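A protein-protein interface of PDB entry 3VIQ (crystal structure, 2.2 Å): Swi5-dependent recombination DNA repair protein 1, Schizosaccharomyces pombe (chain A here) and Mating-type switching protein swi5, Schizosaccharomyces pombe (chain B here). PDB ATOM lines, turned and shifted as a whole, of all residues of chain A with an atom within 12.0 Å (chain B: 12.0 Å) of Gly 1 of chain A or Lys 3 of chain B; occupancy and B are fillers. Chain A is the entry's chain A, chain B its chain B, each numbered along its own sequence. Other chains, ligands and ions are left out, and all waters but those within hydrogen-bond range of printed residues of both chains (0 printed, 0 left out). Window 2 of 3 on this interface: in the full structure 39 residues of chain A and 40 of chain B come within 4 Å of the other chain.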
ATOM      1  N   GLY A   1      17.534 -10.732   3.658  1.00  0.00           N
ATOM      2  CA  GLY A   1      16.107 -10.316   3.802  1.00  0.00           C
ATOM      3  C   GLY A   1      15.619  -9.403   2.698  1.00  0.00           C
ATOM      4  O   GLY A   1      16.395  -8.967   1.863  1.00  0.00           O
ATOM      5  N   HIS A   2      14.311  -9.125   2.699  1.00  0.00           N
ATOM      6  CA  HIS A   2      13.725  -8.168   1.766  1.00  0.00           C
ATOM      7  C   HIS A   2      12.732  -7.143   2.351  1.00  0.00           C
ATOM      8  O   HIS A   2      12.214  -6.312   1.600  1.00  0.00           O
ATOM      9  CB  HIS A   2      13.066  -8.915   0.589  1.00  0.00           C
ATOM     10  CG  HIS A   2      11.904  -9.769   0.972  1.00  0.00           C
ATOM     11  ND1 HIS A   2      12.032 -11.108   1.251  1.00  0.00           N
ATOM     12  CD2 HIS A   2      10.590  -9.482   1.115  1.00  0.00           C
ATOM     13  CE1 HIS A   2      10.852 -11.611   1.557  1.00  0.00           C
ATOM     14  NE2 HIS A   2       9.956 -10.645   1.479  1.00  0.00           N
ATOM     15  N   MET A   3      12.469  -7.185   3.665  1.00  0.00           N
ATOM     16  CA  MET A   3      11.475  -6.277   4.280  1.00  0.00           C
ATOM     17  C   MET A   3      11.931  -4.848   4.294  1.00  0.00           C
ATOM     18  O   MET A   3      11.094  -3.964   4.281  1.00  0.00           O
ATOM     19  CB  MET A   3      11.116  -6.651   5.723  1.00  0.00           C
ATOM     20  CG  MET A   3      10.232  -7.860   5.867  1.00  0.00           C
ATOM     21  SD  MET A   3       8.674  -7.703   4.985  1.00  0.00           S
ATOM     22  CE  MET A   3       7.890  -6.426   5.981  1.00  0.00           C
ATOM     23  N   GLN A   4      13.242  -4.600   4.338  1.00  0.00           N
ATOM     24  CA  GLN A   4      13.714  -3.217   4.249  1.00  0.00           C
ATOM     25  C   GLN A   4      13.356  -2.707   2.881  1.00  0.00           C
ATOM     26  O   GLN A   4      12.920  -1.572   2.749  1.00  0.00           O
ATOM     27  CB  GLN A   4      15.219  -3.054   4.582  1.00  0.00           C
ATOM     28  CG  GLN A   4      15.500  -3.343   6.071  1.00  0.00           C
ATOM     29  CD  GLN A   4      16.981  -3.233   6.487  1.00  0.00           C
ATOM     30  OE1 GLN A   4      17.797  -2.587   5.836  1.00  0.00           O
ATOM     31  NE2 GLN A   4      17.306  -3.841   7.604  1.00  0.00           N
ATOM     32  N   LEU A   5      13.475  -3.551   1.856  1.00  0.00           N
ATOM     33  CA  LEU A   5      13.153  -3.084   0.485  1.00  0.00           C
ATOM     34  C   LEU A   5      11.653  -2.824   0.302  1.00  0.00           C
ATOM     35  O   LEU A   5      11.270  -1.881  -0.377  1.00  0.00           O
ATOM     36  CB  LEU A   5      13.656  -4.054  -0.591  1.00  0.00           C
ATOM     37  CG  LEU A   5      15.128  -4.038  -0.973  1.00  0.00           C
ATOM     38  CD1 LEU A   5      15.458  -5.354  -1.675  1.00  0.00           C
ATOM     39  CD2 LEU A   5      15.536  -2.835  -1.850  1.00  0.00           C
ATOM     40  N   LEU A   6      10.828  -3.701   0.870  1.00  0.00           N
ATOM     41  CA  LEU A   6       9.386  -3.575   0.803  1.00  0.00           C
ATOM     42  C   LEU A   6       8.931  -2.297   1.490  1.00  0.00           C
ATOM     43  O   LEU A   6       8.029  -1.596   1.021  1.00  0.00           O
ATOM     44  CB  LEU A   6       8.687  -4.747   1.478  1.00  0.00           C
ATOM     45  CG  LEU A   6       8.377  -5.964   0.600  1.00  0.00           C
ATOM     46  CD1 LEU A   6       7.788  -7.051   1.469  1.00  0.00           C
ATOM     47  CD2 LEU A   6       7.438  -5.591  -0.541  1.00  0.00           C
ATOM     48  N   SER A   7       9.564  -1.997   2.604  1.00  0.00           N
ATOM     49  CA  SER A   7       9.193  -0.820   3.354  1.00  0.00           C
ATOM     50  C   SER A   7       9.632   0.429   2.594  1.00  0.00           C
ATOM     51  O   SER A   7       8.932   1.423   2.570  1.00  0.00           O
ATOM     52  CB  SER A   7       9.784  -0.887   4.750  1.00  0.00           C
ATOM     53  OG  SER A   7       9.696   0.390   5.318  1.00  0.00           O
ATOM     54  N   ARG A   8      10.764   0.351   1.919  1.00  0.00           N
ATOM     55  CA  ARG A   8      11.244   1.486   1.144  1.00  0.00           C
ATOM     56  C   ARG A   8      10.413   1.661  -0.129  1.00  0.00           C
ATOM     57  O   ARG A   8      10.161   2.780  -0.527  1.00  0.00           O
ATOM     58  CB  ARG A   8      12.717   1.314   0.830  1.00  0.00           C
ATOM     59  CG  ARG A   8      13.361   2.408   0.044  1.00  0.00           C
ATOM     60  CD  ARG A   8      14.873   2.103  -0.122  1.00  0.00           C
ATOM     61  NE  ARG A   8      15.517   3.115  -0.945  1.00  0.00           N
ATOM     62  CZ  ARG A   8      16.002   4.267  -0.476  1.00  0.00           C
ATOM     63  NH1 ARG A   8      15.942   4.568   0.835  1.00  0.00           N
ATOM     64  NH2 ARG A   8      16.565   5.131  -1.317  1.00  0.00           N
ATOM     65  N   ARG A   9       9.967   0.575  -0.756  1.00  0.00           N
ATOM     66  CA  ARG A   9       9.066   0.732  -1.902  1.00  0.00           C
ATOM     67  C   ARG A   9       7.803   1.521  -1.517  1.00  0.00           C
ATOM     68  O   ARG A   9       7.370   2.393  -2.251  1.00  0.00           O
ATOM     69  CB  ARG A   9       8.655  -0.615  -2.486  1.00  0.00           C
ATOM     70  CG  ARG A   9       7.691  -0.518  -3.670  1.00  0.00           C
ATOM     71  CD  ARG A   9       7.454  -1.912  -4.347  1.00  0.00           C
ATOM     72  NE  ARG A   9       6.698  -2.806  -3.499  1.00  0.00           N
ATOM     73  CZ  ARG A   9       6.280  -4.038  -3.826  1.00  0.00           C
ATOM     74  NH1 ARG A   9       6.529  -4.563  -5.018  1.00  0.00           N
ATOM     75  NH2 ARG A   9       5.597  -4.748  -2.932  1.00  0.00           N
ATOM     76  N   MET B   1       8.144 -12.542  -6.442  1.00  0.00           N
ATOM     77  CA  MET B   1       9.182 -11.565  -6.875  1.00  0.00           C
ATOM     78  C   MET B   1      10.516 -11.860  -6.171  1.00  0.00           C
ATOM     79  O   MET B   1      10.579 -11.875  -4.954  1.00  0.00           O
ATOM     80  CB  MET B   1       8.701 -10.134  -6.564  1.00  0.00           C
ATOM     81  CG  MET B   1       9.512  -9.032  -7.226  1.00  0.00           C
ATOM     82  SD  MET B   1       8.627  -7.470  -7.527  1.00  0.00           S
ATOM     83  CE  MET B   1       9.727  -6.787  -8.735  1.00  0.00           C
ATOM     84  N   GLU B   2      11.578 -12.094  -6.935  1.00  0.00           N
ATOM     85  CA  GLU B   2      12.915 -12.233  -6.345  1.00  0.00           C
ATOM     86  C   GLU B   2      13.360 -10.882  -5.758  1.00  0.00           C
ATOM     87  O   GLU B   2      12.826  -9.818  -6.115  1.00  0.00           O
ATOM     88  CB  GLU B   2      13.955 -12.670  -7.385  1.00  0.00           C
ATOM     89  CG  GLU B   2      13.605 -13.904  -8.220  1.00  0.00           C
ATOM     90  CD  GLU B   2      13.710 -15.191  -7.440  1.00  0.00           C
ATOM     91  OE1 GLU B   2      13.040 -15.310  -6.394  1.00  0.00           O
ATOM     92  OE2 GLU B   2      14.457 -16.094  -7.877  1.00  0.00           O
ATOM     93  N   LYS B   3      14.356 -10.944  -4.882  1.00  0.00           N
ATOM     94  CA  LYS B   3      14.916  -9.767  -4.223  1.00  0.00           C
ATOM     95  C   LYS B   3      15.465  -8.810  -5.283  1.00  0.00           C
ATOM     96  O   LYS B   3      15.214  -7.615  -5.219  1.00  0.00           O
ATOM     97  CB  LYS B   3      16.023 -10.164  -3.230  1.00  0.00           C
ATOM     98  CG  LYS B   3      16.305  -9.089  -2.218  1.00  0.00           C
ATOM     99  CD  LYS B   3      17.468  -9.444  -1.300  1.00  0.00           C
ATOM    100  CE  LYS B   3      18.067  -8.193  -0.669  1.00  0.00           C
ATOM    101  NZ  LYS B   3      18.717  -8.537   0.628  1.00  0.00           N
ATOM    102  N   SER B   4      16.193  -9.374  -6.243  1.00  0.00           N
ATOM    103  CA  SER B   4      16.673  -8.697  -7.433  1.00  0.00           C
ATOM    104  C   SER B   4      15.630  -7.851  -8.138  1.00  0.00           C
ATOM    105  O   SER B   4      15.873  -6.691  -8.473  1.00  0.00           O
ATOM    106  CB  SER B   4      17.160  -9.740  -8.448  1.00  0.00           C
ATOM    107  OG  SER B   4      18.481 -10.109  -8.158  1.00  0.00           O
ATOM    108  N   GLN B   5      14.496  -8.475  -8.420  1.00  0.00           N
ATOM    109  CA  GLN B   5      13.405  -7.797  -9.085  1.00  0.00           C
ATOM    110  C   GLN B   5      12.884  -6.662  -8.216  1.00  0.00           C
ATOM    111  O   GLN B   5      12.575  -5.593  -8.722  1.00  0.00           O
ATOM    112  CB  GLN B   5      12.287  -8.776  -9.385  1.00  0.00           C
ATOM    113  CG  GLN B   5      12.705  -9.912 -10.338  1.00  0.00           C
ATOM    114  CD  GLN B   5      11.605 -10.947 -10.547  1.00  0.00           C
ATOM    115  OE1 GLN B   5      10.847 -11.277  -9.629  1.00  0.00           O
ATOM    116  NE2 GLN B   5      11.521 -11.468 -11.759  1.00  0.00           N
ATOM    117  N   LEU B   6      12.820  -6.883  -6.906  1.00  0.00           N
ATOM    118  CA  LEU B   6      12.314  -5.870  -5.997  1.00  0.00           C
ATOM    119  C   LEU B   6      13.291  -4.666  -5.916  1.00  0.00           C
ATOM    120  O   LEU B   6      12.874  -3.514  -5.930  1.00  0.00           O
ATOM    121  CB  LEU B   6      12.036  -6.490  -4.618  1.00  0.00           C
ATOM    122  CG  LEU B   6      11.540  -5.499  -3.584  1.00  0.00           C
ATOM    123  CD1 LEU B   6      10.274  -4.828  -4.088  1.00  0.00           C
ATOM    124  CD2 LEU B   6      11.337  -6.151  -2.227  1.00  0.00           C
ATOM    125  N   GLU B   7      14.588  -4.961  -5.879  1.00  0.00           N
ATOM    126  CA  GLU B   7      15.639  -3.939  -6.006  1.00  0.00           C
ATOM    127  C   GLU B   7      15.469  -3.127  -7.271  1.00  0.00           C
ATOM    128  O   GLU B   7      15.677  -1.917  -7.255  1.00  0.00           O
ATOM    129  CB  GLU B   7      17.052  -4.587  -6.015  1.00  0.00           C
ATOM    130  CG  GLU B   7      17.611  -4.826  -4.624  1.00  0.00           C
ATOM    131  CD  GLU B   7      18.696  -5.918  -4.520  1.00  0.00           C
ATOM    132  OE1 GLU B   7      19.130  -6.499  -5.552  1.00  0.00           O
ATOM    133  OE2 GLU B   7      19.140  -6.168  -3.368  1.00  0.00           O
ATOM    134  N   SER B   8      15.140  -3.786  -8.384  1.00  0.00           N
ATOM    135  CA  SER B   8      14.910  -3.045  -9.616  1.00  0.00           C
ATOM    136  C   SER B   8      13.715  -2.125  -9.507  1.00  0.00           C
ATOM    137  O   SER B   8      13.814  -0.975  -9.906  1.00  0.00           O
ATOM    138  CB  SER B   8      14.772  -3.971 -10.822  1.00  0.00           C
ATOM    139  OG  SER B   8      16.041  -4.520 -11.141  1.00  0.00           O
ATOM    140  N   ARG B   9      12.602  -2.579  -8.927  1.00  0.00           N
ATOM    141  CA  ARG B   9      11.454  -1.664  -8.773  1.00  0.00           C
ATOM    142  C   ARG B   9      11.785  -0.483  -7.861  1.00  0.00           C
ATOM    143  O   ARG B   9      11.377   0.651  -8.111  1.00  0.00           O
ATOM    144  CB  ARG B   9      10.214  -2.393  -8.253  1.00  0.00           C
ATOM    145  CG  ARG B   9       9.793  -3.579  -9.167  1.00  0.00           C
ATOM    146  CD  ARG B   9       9.122  -3.058 -10.413  1.00  0.00           C
ATOM    147  NE  ARG B   9       7.877  -2.389 -10.066  1.00  0.00           N
ATOM    148  CZ  ARG B   9       7.174  -1.604 -10.871  1.00  0.00           C
ATOM    149  NH1 ARG B   9       7.577  -1.362 -12.122  1.00  0.00           N
ATOM    150  NH2 ARG B   9       6.052  -1.061 -10.410  1.00  0.00           N
ATOM    151  N   VAL B  10      12.533  -0.746  -6.799  1.00  0.00           N
ATOM    152  CA  VAL B  10      12.883   0.300  -5.831  1.00  0.00           C
ATOM    153  C   VAL B  10      13.787   1.325  -6.523  1.00  0.00           C
ATOM    154  O   VAL B  10      13.566   2.506  -6.358  1.00  0.00           O
ATOM    155  CB  VAL B  10      13.525  -0.283  -4.564  1.00  0.00           C
ATOM    156  CG1 VAL B  10      14.266   0.785  -3.758  1.00  0.00           C
ATOM    157  CG2 VAL B  10      12.464  -0.976  -3.713  1.00  0.00           C
ATOM    158  N   HIS B  11      14.746   0.883  -7.346  1.00  0.00           N
ATOM    159  CA  HIS B  11      15.628   1.831  -8.036  1.00  0.00           C
ATOM    160  C   HIS B  11      14.853   2.656  -9.092  1.00  0.00           C
ATOM    161  O   HIS B  11      15.108   3.854  -9.245  1.00  0.00           O
ATOM    162  CB  HIS B  11      16.886   1.167  -8.681  1.00  0.00           C
ATOM    163  CG  HIS B  11      17.922   0.686  -7.685  1.00  0.00           C
ATOM    164  ND1 HIS B  11      18.415   1.477  -6.663  1.00  0.00           N
ATOM    165  CD2 HIS B  11      18.585  -0.499  -7.590  1.00  0.00           C
ATOM    166  CE1 HIS B  11      19.311   0.791  -5.968  1.00  0.00           C
ATOM    167  NE2 HIS B  11      19.437  -0.407  -6.513  1.00  0.00           N
ATOM    168  N   LEU B  12      13.905   2.049  -9.796  1.00  0.00           N
ATOM    169  CA  LEU B  12      13.023   2.836 -10.669  1.00  0.00           C
ATOM    170  C   LEU B  12      12.209   3.911  -9.916  1.00  0.00           C
ATOM    171  O   LEU B  12      12.055   5.033 -10.402  1.00  0.00           O
ATOM    172  CB  LEU B  12      12.088   1.924 -11.443  1.00  0.00           C
ATOM    173  CG  LEU B  12      12.813   1.083 -12.492  1.00  0.00           C
ATOM    174  CD1 LEU B  12      11.928  -0.086 -12.940  1.00  0.00           C
ATOM    175  CD2 LEU B  12      13.237   2.012 -13.683  1.00  0.00           C
ATOM    176  N   LEU B  13      11.758   3.593  -8.708  1.00  0.00           N
ATOM    177  CA  LEU B  13      10.985   4.552  -7.920  1.00  0.00           C
ATOM    178  C   LEU B  13      11.912   5.691  -7.470  1.00  0.00           C
ATOM    179  O   LEU B  13      11.487   6.843  -7.374  1.00  0.00           O
ATOM    180  CB  LEU B  13      10.359   3.849  -6.711  1.00  0.00           C
ATOM    181  CG  LEU B  13       9.082   3.067  -7.064  1.00  0.00           C
ATOM    182  CD1 LEU B  13       8.748   2.035  -5.964  1.00  0.00           C
ATOM    183  CD2 LEU B  13       7.903   4.022  -7.295  1.00  0.00           C
ATOM    184  N   GLU B  14      13.177   5.361  -7.197  1.00  0.00           N
ATOM    185  CA  GLU B  14      14.125   6.360  -6.781  1.00  0.00           C
ATOM    186  C   GLU B  14      14.286   7.330  -7.924  1.00  0.00           C
ATOM    187  O   GLU B  14      14.234   8.517  -7.701  1.00  0.00           O
ATOM    188  CB  GLU B  14      15.477   5.767  -6.383  1.00  0.00           C
ATOM    189  CG  GLU B  14      15.481   5.154  -5.004  1.00  0.00           C
ATOM    190  CD  GLU B  14      16.668   4.234  -4.715  1.00  0.00           C
ATOM    191  OE1 GLU B  14      17.498   3.934  -5.601  1.00  0.00           O
ATOM    192  OE2 GLU B  14      16.764   3.786  -3.556  1.00  0.00           O
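NZ of Lys 3 of chain B sits at hydrogen-bond distance from O of Gly 1 of chain A (2.7 Å). The guanidinium group (NH2) of Arg 8 of chain A is in salt-bridge range of the side-chain carboxylate (OE2) of Glu 14 of chain B (2.6 Å).
OE1 of Glu 14 of chain B lies within hydrogen-bond range of ND1 of His 11 of chain B.
CD2 of Leu 6 of chain B touches O of His 2 of chain A (3.9 Å). Leu 5 of chain A touches Lys 3 of chain B (CD1 to CG, 3.9 Å). CB of Leu 5 of chain A touches CD2 of Leu 6 of chain B, at 3.5 Å. Leu 5 of chain A touches Glu 7 of chain B. CG2 of Val 10 of chain B touches O of Leu 5 of chain A (3.7 Å). Leu 6 of chain B touches Leu 6 of chain A (CD2 to N, 3.98 Å). Arg 8 of chain A touches Val 10 of chain B. Arg 9 of chain A touches Leu 6 of chain B. Leu 13 of chain B touches Arg 9 of chain A.
Gly 1 of chain A touches one residue of chain B. Of chain A, only Gly 1 and Leu 5 come within 4 Å of Lys 3 of chain B. Of chain B, only Leu 6 (3.9 Å) comes within 4 Å of His 2 of chain A. No residue of chain A comes within 4 Å of Glu 2 of chain B. No residue of chain A comes within 4 Å of Ser 4 of chain B. Gln 5 of chain B touches none of the printed residues of chain A. Of chain A, only Leu 5 (3.7 Å) comes within 4 Å of Glu 7 of chain B. Of the printed residues of chain A, Glu 14 of chain B touches Arg 8. Of the printed residues of chain B, Leu 6 of chain A touches Leu 6. Of the printed residues of chain A, Leu 13 of chain B touches Arg 9. The nearest residue of chain B that does not touch Gly 1 of chain A is Glu 7 of chain B (6.5 Å). The nearest printed residue of chain A that does not touch Leu 6 of chain B is Met 3 of chain A (6.1 Å).
Hydrophobic or aromatic side chains of chain A within 4 Å of the printed part of chain B: Leu 5. Along chain A the printed residues that touch a printed residue of chain B span positions 1 to 9. Of the 14 printed residues of chain B, 6 touch a printed residue of chain A. Hydrophobic or aromatic side chains of chain B that line the printed part of chain A: Leu 6, Val 10 and Leu 13.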
